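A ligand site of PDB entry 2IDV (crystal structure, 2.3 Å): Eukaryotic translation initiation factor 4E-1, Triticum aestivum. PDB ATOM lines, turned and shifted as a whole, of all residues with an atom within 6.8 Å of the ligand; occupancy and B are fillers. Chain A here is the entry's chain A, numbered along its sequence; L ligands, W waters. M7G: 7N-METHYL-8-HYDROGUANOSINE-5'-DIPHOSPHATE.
The guanidinium group (NH1) of Arg 20 lies within salt-bridge range of an oxygen (O1B) of the ligand (2.5 Å). An oxygen (O2B) of the ligand lies within salt-bridge range of the guanidinium group (NE) of Arg 120 (2.6 Å). OE2 of Glu 71 sits at hydrogen-bond distance from N2 of the ligand, at 2.9 Å. The backbone NH (N) of Trp 70 is in hydrogen-bond range of an oxygen (O6) of the ligand, 3.0 Å away. O2B of the ligand is in salt-bridge range of NH2 of Arg 125 (3.2 Å).
The side-chain carboxylate of Asp 58 lies within salt-bridge range of the guanidinium group of Arg 120, 3.2 Å away. The backbone carbonyl oxygen of Arg 125 is in hydrogen-bond range of the backbone NH of Ser 118 (2.7 Å).
Residues that only touch the ligand: Gln 21 (3.8 Å), Trp 24 (3.1 Å) and Lys 69 (3.5 Å). Hydrophobic or aromatic side chains within 4 Å of the ligand: Trp 24 and Trp 70. Within 4 Å of the ligand: Arg 20, Gln 21, Trp 24, Lys 69, Trp 70, Glu 71, Arg 120 and Arg 125. Along chain A the residues within 4 Å of the ligand span positions 20 to 125.
Water W3 lies within hydrogen-bond range of an oxygen (O3') of the ligand (2.7 Å), the backbone carbonyl oxygen (O) of Ala 164 (2.9 Å) and the backbone carbonyl oxygen (O) of Arg 166 (3.3 Å). Water W5 bridges OD2 of Asp 58 (2.6 Å) and O2A of the ligand (2.9 Å). Water W2 bridges the side-chain carboxylate of Glu 71 and a nitrogen (N2) of the ligand. Water W6 lies within hydrogen-bond range of the guanidinium group of Arg 125 (2.9 Å), the side-chain hydroxyl of Ser 118 (3.4 Å) and an oxygen (O2A) of the ligand (3.4 Å).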
ATOM      1  N   ARG A  20       8.778  -2.995  -4.114  1.00  0.00           N
ATOM      2  CA  ARG A  20       9.659  -1.825  -4.004  1.00  0.00           C
ATOM      3  C   ARG A  20      10.271  -1.684  -2.611  1.00  0.00           C
ATOM      4  O   ARG A  20      11.125  -0.821  -2.374  1.00  0.00           O
ATOM      5  CB  ARG A  20       8.876  -0.557  -4.382  1.00  0.00           C
ATOM      6  CG  ARG A  20       8.721  -0.369  -5.900  1.00  0.00           C
ATOM      7  CD  ARG A  20       8.005   0.919  -6.287  1.00  0.00           C
ATOM      8  NE  ARG A  20       6.569   0.723  -6.421  1.00  0.00           N
ATOM      9  CZ  ARG A  20       5.717   0.652  -5.405  1.00  0.00           C
ATOM     10  NH1 ARG A  20       6.139   0.765  -4.162  1.00  0.00           N
ATOM     11  NH2 ARG A  20       4.426   0.446  -5.643  1.00  0.00           N
ATOM     12  N   GLN A  21       9.843  -2.548  -1.694  1.00  0.00           N
ATOM     13  CA  GLN A  21      10.349  -2.520  -0.332  1.00  0.00           C
ATOM     14  C   GLN A  21      11.669  -3.262  -0.218  1.00  0.00           C
ATOM     15  O   GLN A  21      12.438  -3.012   0.703  1.00  0.00           O
ATOM     16  CB  GLN A  21       9.338  -3.142   0.636  1.00  0.00           C
ATOM     17  CG  GLN A  21       7.912  -2.635   0.471  1.00  0.00           C
ATOM     18  CD  GLN A  21       7.792  -1.126   0.598  1.00  0.00           C
ATOM     19  OE1 GLN A  21       8.257  -0.529   1.567  1.00  0.00           O
ATOM     20  NE2 GLN A  21       7.150  -0.502  -0.389  1.00  0.00           N
ATOM     21  N   VAL A  22      11.942  -4.168  -1.144  1.00  0.00           N
ATOM     22  CA  VAL A  22      13.199  -4.907  -1.067  1.00  0.00           C
ATOM     23  C   VAL A  22      14.218  -4.406  -2.087  1.00  0.00           C
ATOM     24  O   VAL A  22      13.913  -4.255  -3.266  1.00  0.00           O
ATOM     25  CB  VAL A  22      12.970  -6.434  -1.255  1.00  0.00           C
ATOM     26  CG1 VAL A  22      11.543  -6.825  -0.845  1.00  0.00           C
ATOM     27  CG2 VAL A  22      13.240  -6.839  -2.684  1.00  0.00           C
ATOM     28  N   TRP A  24      15.455  -1.506  -2.835  1.00  0.00           N
ATOM     29  CA  TRP A  24      14.917  -0.399  -3.599  1.00  0.00           C
ATOM     30  C   TRP A  24      15.937   0.216  -4.547  1.00  0.00           C
ATOM     31  O   TRP A  24      17.123   0.287  -4.245  1.00  0.00           O
ATOM     32  CB  TRP A  24      14.392   0.694  -2.673  1.00  0.00           C
ATOM     33  CG  TRP A  24      13.923   1.891  -3.438  1.00  0.00           C
ATOM     34  CD1 TRP A  24      12.692   2.077  -4.013  1.00  0.00           C
ATOM     35  CD2 TRP A  24      14.703   3.044  -3.788  1.00  0.00           C
ATOM     36  NE1 TRP A  24      12.664   3.271  -4.703  1.00  0.00           N
ATOM     37  CE2 TRP A  24      13.890   3.883  -4.569  1.00  0.00           C
ATOM     38  CE3 TRP A  24      16.015   3.444  -3.502  1.00  0.00           C
ATOM     39  CZ2 TRP A  24      14.348   5.112  -5.079  1.00  0.00           C
ATOM     40  CZ3 TRP A  24      16.473   4.658  -4.012  1.00  0.00           C
ATOM     41  CH2 TRP A  24      15.640   5.475  -4.786  1.00  0.00           C
ATOM     42  N   GLY A  25      15.456   0.666  -5.708  1.00  0.00           N
ATOM     43  CA  GLY A  25      16.319   1.291  -6.690  1.00  0.00           C
ATOM     44  C   GLY A  25      17.603   0.573  -7.057  1.00  0.00           C
ATOM     45  O   GLY A  25      18.595   1.224  -7.390  1.00  0.00           O
ATOM     46  N   GLY A  56       4.242   1.016 -10.706  1.00  0.00           N
ATOM     47  CA  GLY A  56       5.515   0.790 -10.045  1.00  0.00           C
ATOM     48  C   GLY A  56       6.707   1.525 -10.658  1.00  0.00           C
ATOM     49  O   GLY A  56       7.694   1.754  -9.973  1.00  0.00           O
ATOM     50  N   ASP A  58       9.138   4.500 -12.096  1.00  0.00           N
ATOM     51  CA  ASP A  58       9.454   5.885 -11.707  1.00  0.00           C
ATOM     52  C   ASP A  58      10.332   6.568 -12.775  1.00  0.00           C
ATOM     53  O   ASP A  58      11.348   6.022 -13.223  1.00  0.00           O
ATOM     54  CB  ASP A  58      10.190   5.950 -10.353  1.00  0.00           C
ATOM     55  CG  ASP A  58       9.249   5.774  -9.169  1.00  0.00           C
ATOM     56  OD1 ASP A  58       8.206   6.459  -9.098  1.00  0.00           O
ATOM     57  OD2 ASP A  58       9.572   4.950  -8.284  1.00  0.00           O
ATOM     58  N   PRO A  68      18.450  10.611  -8.048  1.00  0.00           N
ATOM     59  CA  PRO A  68      17.110  10.518  -7.467  1.00  0.00           C
ATOM     60  C   PRO A  68      17.026   9.630  -6.225  1.00  0.00           C
ATOM     61  O   PRO A  68      16.218   8.694  -6.174  1.00  0.00           O
ATOM     62  CB  PRO A  68      16.278   9.943  -8.619  1.00  0.00           C
ATOM     63  CG  PRO A  68      17.016  10.360  -9.839  1.00  0.00           C
ATOM     64  CD  PRO A  68      18.448  10.102  -9.428  1.00  0.00           C
ATOM     65  N   LYS A  69      17.840   9.955  -5.229  1.00  0.00           N
ATOM     66  CA  LYS A  69      17.865   9.196  -3.972  1.00  0.00           C
ATOM     67  C   LYS A  69      17.987  10.081  -2.727  1.00  0.00           C
ATOM     68  O   LYS A  69      18.755  11.051  -2.704  1.00  0.00           O
ATOM     69  CB  LYS A  69      19.011   8.186  -4.006  1.00  0.00           C
ATOM     70  CG  LYS A  69      18.749   7.029  -4.972  1.00  0.00           C
ATOM     71  CD  LYS A  69      19.983   6.173  -5.245  1.00  0.00           C
ATOM     72  CE  LYS A  69      20.819   6.710  -6.413  1.00  0.00           C
ATOM     73  NZ  LYS A  69      21.632   5.631  -7.072  1.00  0.00           N
ATOM     74  N   TRP A  70      17.226   9.747  -1.694  1.00  0.00           N
ATOM     75  CA  TRP A  70      17.286  10.522  -0.453  1.00  0.00           C
ATOM     76  C   TRP A  70      18.713  10.520   0.120  1.00  0.00           C
ATOM     77  O   TRP A  70      19.187  11.534   0.635  1.00  0.00           O
ATOM     78  CB  TRP A  70      16.346   9.934   0.596  1.00  0.00           C
ATOM     79  CG  TRP A  70      14.902   9.858   0.178  1.00  0.00           C
ATOM     80  CD1 TRP A  70      14.233  10.772  -0.576  1.00  0.00           C
ATOM     81  CD2 TRP A  70      13.945   8.863   0.556  1.00  0.00           C
ATOM     82  NE1 TRP A  70      12.910  10.407  -0.693  1.00  0.00           N
ATOM     83  CE2 TRP A  70      12.709   9.240   0.000  1.00  0.00           C
ATOM     84  CE3 TRP A  70      14.015   7.687   1.314  1.00  0.00           C
ATOM     85  CZ2 TRP A  70      11.536   8.476   0.166  1.00  0.00           C
ATOM     86  CZ3 TRP A  70      12.849   6.924   1.488  1.00  0.00           C
ATOM     87  CH2 TRP A  70      11.631   7.331   0.913  1.00  0.00           C
ATOM     88  N   GLU A  71      19.389   9.377   0.021  1.00  0.00           N
ATOM     89  CA  GLU A  71      20.744   9.220   0.535  1.00  0.00           C
ATOM     90  C   GLU A  71      21.782  10.121  -0.139  1.00  0.00           C
ATOM     91  O   GLU A  71      22.904  10.239   0.338  1.00  0.00           O
ATOM     92  CB  GLU A  71      21.184   7.763   0.426  1.00  0.00           C
ATOM     93  CG  GLU A  71      21.266   7.224  -0.999  1.00  0.00           C
ATOM     94  CD  GLU A  71      20.309   6.084  -1.245  1.00  0.00           C
ATOM     95  OE1 GLU A  71      20.593   5.250  -2.132  1.00  0.00           O
ATOM     96  OE2 GLU A  71      19.252   6.019  -0.571  1.00  0.00           O
ATOM     97  N   LYS A  80      10.371  17.351  -0.454  1.00  0.00           N
ATOM     98  CA  LYS A  80       9.732  17.407  -1.756  1.00  0.00           C
ATOM     99  C   LYS A  80       8.283  17.843  -1.720  1.00  0.00           C
ATOM    100  O   LYS A  80       7.579  17.605  -0.732  1.00  0.00           O
ATOM    101  CB  LYS A  80       9.766  16.039  -2.422  1.00  0.00           C
ATOM    102  CG  LYS A  80       8.959  14.970  -1.674  1.00  0.00           C
ATOM    103  CD  LYS A  80       8.780  13.721  -2.534  1.00  0.00           C
ATOM    104  CE  LYS A  80       7.873  12.666  -1.927  1.00  0.00           C
ATOM    105  NZ  LYS A  80       8.481  12.097  -0.697  1.00  0.00           N
ATOM    106  N   SER A 118       5.762   9.512 -10.364  1.00  0.00           N
ATOM    107  CA  SER A 118       5.552   8.116  -9.973  1.00  0.00           C
ATOM    108  C   SER A 118       4.202   7.571 -10.417  1.00  0.00           C
ATOM    109  O   SER A 118       3.149   8.142 -10.113  1.00  0.00           O
ATOM    110  CB  SER A 118       5.667   7.946  -8.446  1.00  0.00           C
ATOM    111  OG  SER A 118       6.947   8.301  -7.967  1.00  0.00           O
ATOM    112  N   VAL A 119       4.236   6.458 -11.127  1.00  0.00           N
ATOM    113  CA  VAL A 119       3.018   5.830 -11.590  1.00  0.00           C
ATOM    114  C   VAL A 119       2.670   4.661 -10.670  1.00  0.00           C
ATOM    115  O   VAL A 119       3.490   3.777 -10.432  1.00  0.00           O
ATOM    116  CB  VAL A 119       3.176   5.340 -13.034  1.00  0.00           C
ATOM    117  CG1 VAL A 119       2.074   4.352 -13.375  1.00  0.00           C
ATOM    118  CG2 VAL A 119       3.101   6.522 -13.977  1.00  0.00           C
ATOM    119  N   ARG A 120       1.450   4.668 -10.150  1.00  0.00           N
ATOM    120  CA  ARG A 120       1.014   3.598  -9.266  1.00  0.00           C
ATOM    121  C   ARG A 120      -0.358   3.052  -9.650  1.00  0.00           C
ATOM    122  O   ARG A 120      -0.969   3.494 -10.639  1.00  0.00           O
ATOM    123  CB  ARG A 120       1.014   4.100  -7.817  1.00  0.00           C
ATOM    124  CG  ARG A 120       2.399   4.463  -7.284  1.00  0.00           C
ATOM    125  CD  ARG A 120       3.342   3.248  -7.188  1.00  0.00           C
ATOM    126  NE  ARG A 120       4.673   3.607  -6.715  1.00  0.00           N
ATOM    127  CZ  ARG A 120       5.577   4.285  -7.428  1.00  0.00           C
ATOM    128  NH1 ARG A 120       5.308   4.658  -8.667  1.00  0.00           N
ATOM    129  NH2 ARG A 120       6.751   4.598  -6.890  1.00  0.00           N
ATOM    130  N   ARG A 125       1.741  10.498  -9.192  1.00  0.00           N
ATOM    131  CA  ARG A 125       2.193  11.654  -8.438  1.00  0.00           C
ATOM    132  C   ARG A 125       3.384  12.303  -9.099  1.00  0.00           C
ATOM    133  O   ARG A 125       4.254  11.598  -9.605  1.00  0.00           O
ATOM    134  CB  ARG A 125       2.574  11.247  -7.015  1.00  0.00           C
ATOM    135  CG  ARG A 125       1.489  10.456  -6.279  1.00  0.00           C
ATOM    136  CD  ARG A 125       1.874  10.199  -4.829  1.00  0.00           C
ATOM    137  NE  ARG A 125       3.077   9.363  -4.724  1.00  0.00           N
ATOM    138  CZ  ARG A 125       3.042   8.035  -4.683  1.00  0.00           C
ATOM    139  NH1 ARG A 125       1.872   7.406  -4.745  1.00  0.00           N
ATOM    140  NH2 ARG A 125       4.160   7.343  -4.566  1.00  0.00           N
ATOM    141  N   TRP A 129      11.906  17.900  -5.962  1.00  0.00           N
ATOM    142  CA  TRP A 129      12.807  17.771  -4.810  1.00  0.00           C
ATOM    143  C   TRP A 129      13.655  19.009  -4.540  1.00  0.00           C
ATOM    144  O   TRP A 129      14.207  19.605  -5.457  1.00  0.00           O
ATOM    145  CB  TRP A 129      13.726  16.574  -5.045  1.00  0.00           C
ATOM    146  CG  TRP A 129      13.033  15.234  -5.003  1.00  0.00           C
ATOM    147  CD1 TRP A 129      11.697  14.982  -5.210  1.00  0.00           C
ATOM    148  CD2 TRP A 129      13.617  13.966  -4.674  1.00  0.00           C
ATOM    149  NE1 TRP A 129      11.424  13.645  -5.020  1.00  0.00           N
ATOM    150  CE2 TRP A 129      12.593  12.999  -4.696  1.00  0.00           C
ATOM    151  CE3 TRP A 129      14.925  13.557  -4.369  1.00  0.00           C
ATOM    152  CZ2 TRP A 129      12.818  11.641  -4.402  1.00  0.00           C
ATOM    153  CZ3 TRP A 129      15.160  12.199  -4.085  1.00  0.00           C
ATOM    154  CH2 TRP A 129      14.111  11.267  -4.100  1.00  0.00           C
ATOM    155  N   ALA A 164      10.187  10.718   5.288  1.00  0.00           N
ATOM    156  CA  ALA A 164       9.794   9.758   4.265  1.00  0.00           C
ATOM    157  C   ALA A 164      10.494   8.419   4.494  1.00  0.00           C
ATOM    158  O   ALA A 164       9.973   7.352   4.146  1.00  0.00           O
ATOM    159  CB  ALA A 164      10.138  10.301   2.893  1.00  0.00           C
ATOM    160  N   LYS A 165      11.687   8.478   5.099  1.00  0.00           N
ATOM    161  CA  LYS A 165      12.484   7.303   5.405  1.00  0.00           C
ATOM    162  C   LYS A 165      11.746   6.417   6.401  1.00  0.00           C
ATOM    163  O   LYS A 165      11.946   5.198   6.425  1.00  0.00           O
ATOM    164  CB  LYS A 165      13.841   7.728   5.985  1.00  0.00           C
ATOM    165  CG  LYS A 165      14.846   8.221   4.938  1.00  0.00           C
ATOM    166  CD  LYS A 165      16.154   8.643   5.590  1.00  0.00           C
ATOM    167  CE  LYS A 165      17.284   8.819   4.573  1.00  0.00           C
ATOM    168  NZ  LYS A 165      17.015   9.916   3.621  1.00  0.00           N
ATOM    169  N   ARG A 166      10.884   7.025   7.203  1.00  0.00           N
ATOM    170  CA  ARG A 166      10.086   6.306   8.188  1.00  0.00           C
ATOM    171  C   ARG A 166       9.322   5.157   7.553  1.00  0.00           C
ATOM    172  O   ARG A 166       8.302   5.365   6.908  1.00  0.00           O
ATOM    173  CB  ARG A 166       9.083   7.258   8.839  1.00  0.00           C
ATOM    174  CG  ARG A 166       9.510   7.797  10.183  1.00  0.00           C
ATOM    175  CD  ARG A 166       8.941   6.945  11.294  1.00  0.00           C
ATOM    176  NE  ARG A 166       8.845   7.702  12.542  1.00  0.00           N
ATOM    177  CZ  ARG A 166       8.207   7.263  13.619  1.00  0.00           C
ATOM    178  NH1 ARG A 166       7.601   6.086  13.599  1.00  0.00           N
ATOM    179  NH2 ARG A 166       8.171   8.009  14.720  1.00  0.00           N
ATOM    180  N   SER A 167       9.823   3.946   7.763  1.00  0.00           N
ATOM    181  CA  SER A 167       9.208   2.752   7.227  1.00  0.00           C
ATOM    182  C   SER A 167       8.117   2.280   8.202  1.00  0.00           C
ATOM    183  O   SER A 167       7.341   1.366   7.899  1.00  0.00           O
ATOM    184  CB  SER A 167      10.253   1.663   7.033  1.00  0.00           C
HETATM  185  PA  M7G L   1       7.904   4.666  -3.377  1.00  0.00           P
HETATM  186  O1A M7G L   1       7.675   3.561  -4.335  1.00  0.00           O
HETATM  187  O2A M7G L   1       8.482   5.924  -3.890  1.00  0.00           O
HETATM  188  O3A M7G L   1       6.504   5.015  -2.650  1.00  0.00           O
HETATM  189  O5' M7G L   1       8.824   4.141  -2.148  1.00  0.00           O
HETATM  190  PB  M7G L   1       5.258   3.990  -2.752  1.00  0.00           P
HETATM  191  O1B M7G L   1       5.624   2.578  -2.486  1.00  0.00           O
HETATM  192  O2B M7G L   1       4.628   4.216  -4.221  1.00  0.00           O
HETATM  193  O3B M7G L   1       4.154   4.554  -1.714  1.00  0.00           O
HETATM  194  C5' M7G L   1       8.613   2.859  -1.560  1.00  0.00           C
HETATM  195  C4' M7G L   1       9.822   2.481  -0.697  1.00  0.00           C
HETATM  196  O4' M7G L   1      11.034   2.408  -1.474  1.00  0.00           O
HETATM  197  C3' M7G L   1      10.115   3.499   0.398  1.00  0.00           C
HETATM  198  O3' M7G L   1       9.246   3.257   1.509  1.00  0.00           O
HETATM  199  C2' M7G L   1      11.518   3.019   0.771  1.00  0.00           C
HETATM  200  O2' M7G L   1      11.425   1.767   1.439  1.00  0.00           O
HETATM  201  C1' M7G L   1      12.126   2.837  -0.628  1.00  0.00           C
HETATM  202  N9  M7G L   1      12.648   4.127  -1.146  1.00  0.00           N
HETATM  203  C8  M7G L   1      11.965   4.997  -1.898  1.00  0.00           C
HETATM  204  N7  M7G L   1      12.761   6.017  -2.187  1.00  0.00           N
HETATM  205  CM7 M7G L   1      12.389   7.199  -2.983  1.00  0.00           C
HETATM  206  C5  M7G L   1      13.962   5.807  -1.637  1.00  0.00           C
HETATM  207  C6  M7G L   1      15.158   6.523  -1.645  1.00  0.00           C
HETATM  208  O6  M7G L   1      15.249   7.591  -2.245  1.00  0.00           O
HETATM  209  N1  M7G L   1      16.262   5.981  -0.973  1.00  0.00           N
HETATM  210  C2  M7G L   1      16.121   4.761  -0.303  1.00  0.00           C
HETATM  211  N2  M7G L   1      17.162   4.242   0.343  1.00  0.00           N
HETATM  212  N3  M7G L   1      14.952   4.103  -0.324  1.00  0.00           N
HETATM  213  C4  M7G L   1      13.878   4.591  -0.966  1.00  0.00           C
HETATM  214  O   HOH W   1      16.792   1.617   0.951  1.00  0.00           O
HETATM  215  O   HOH W   2      18.015   6.952   1.371  1.00  0.00           O
HETATM  216  O   HOH W   3       9.252   4.592   3.839  1.00  0.00           O
HETATM  217  O   HOH W   4       4.295   6.977  -0.955  1.00  0.00           O
HETATM  218  O   HOH W   5       9.639   6.699  -6.402  1.00  0.00           O
HETATM  219  O   HOH W   6       6.714   8.688  -4.642  1.00  0.00           O
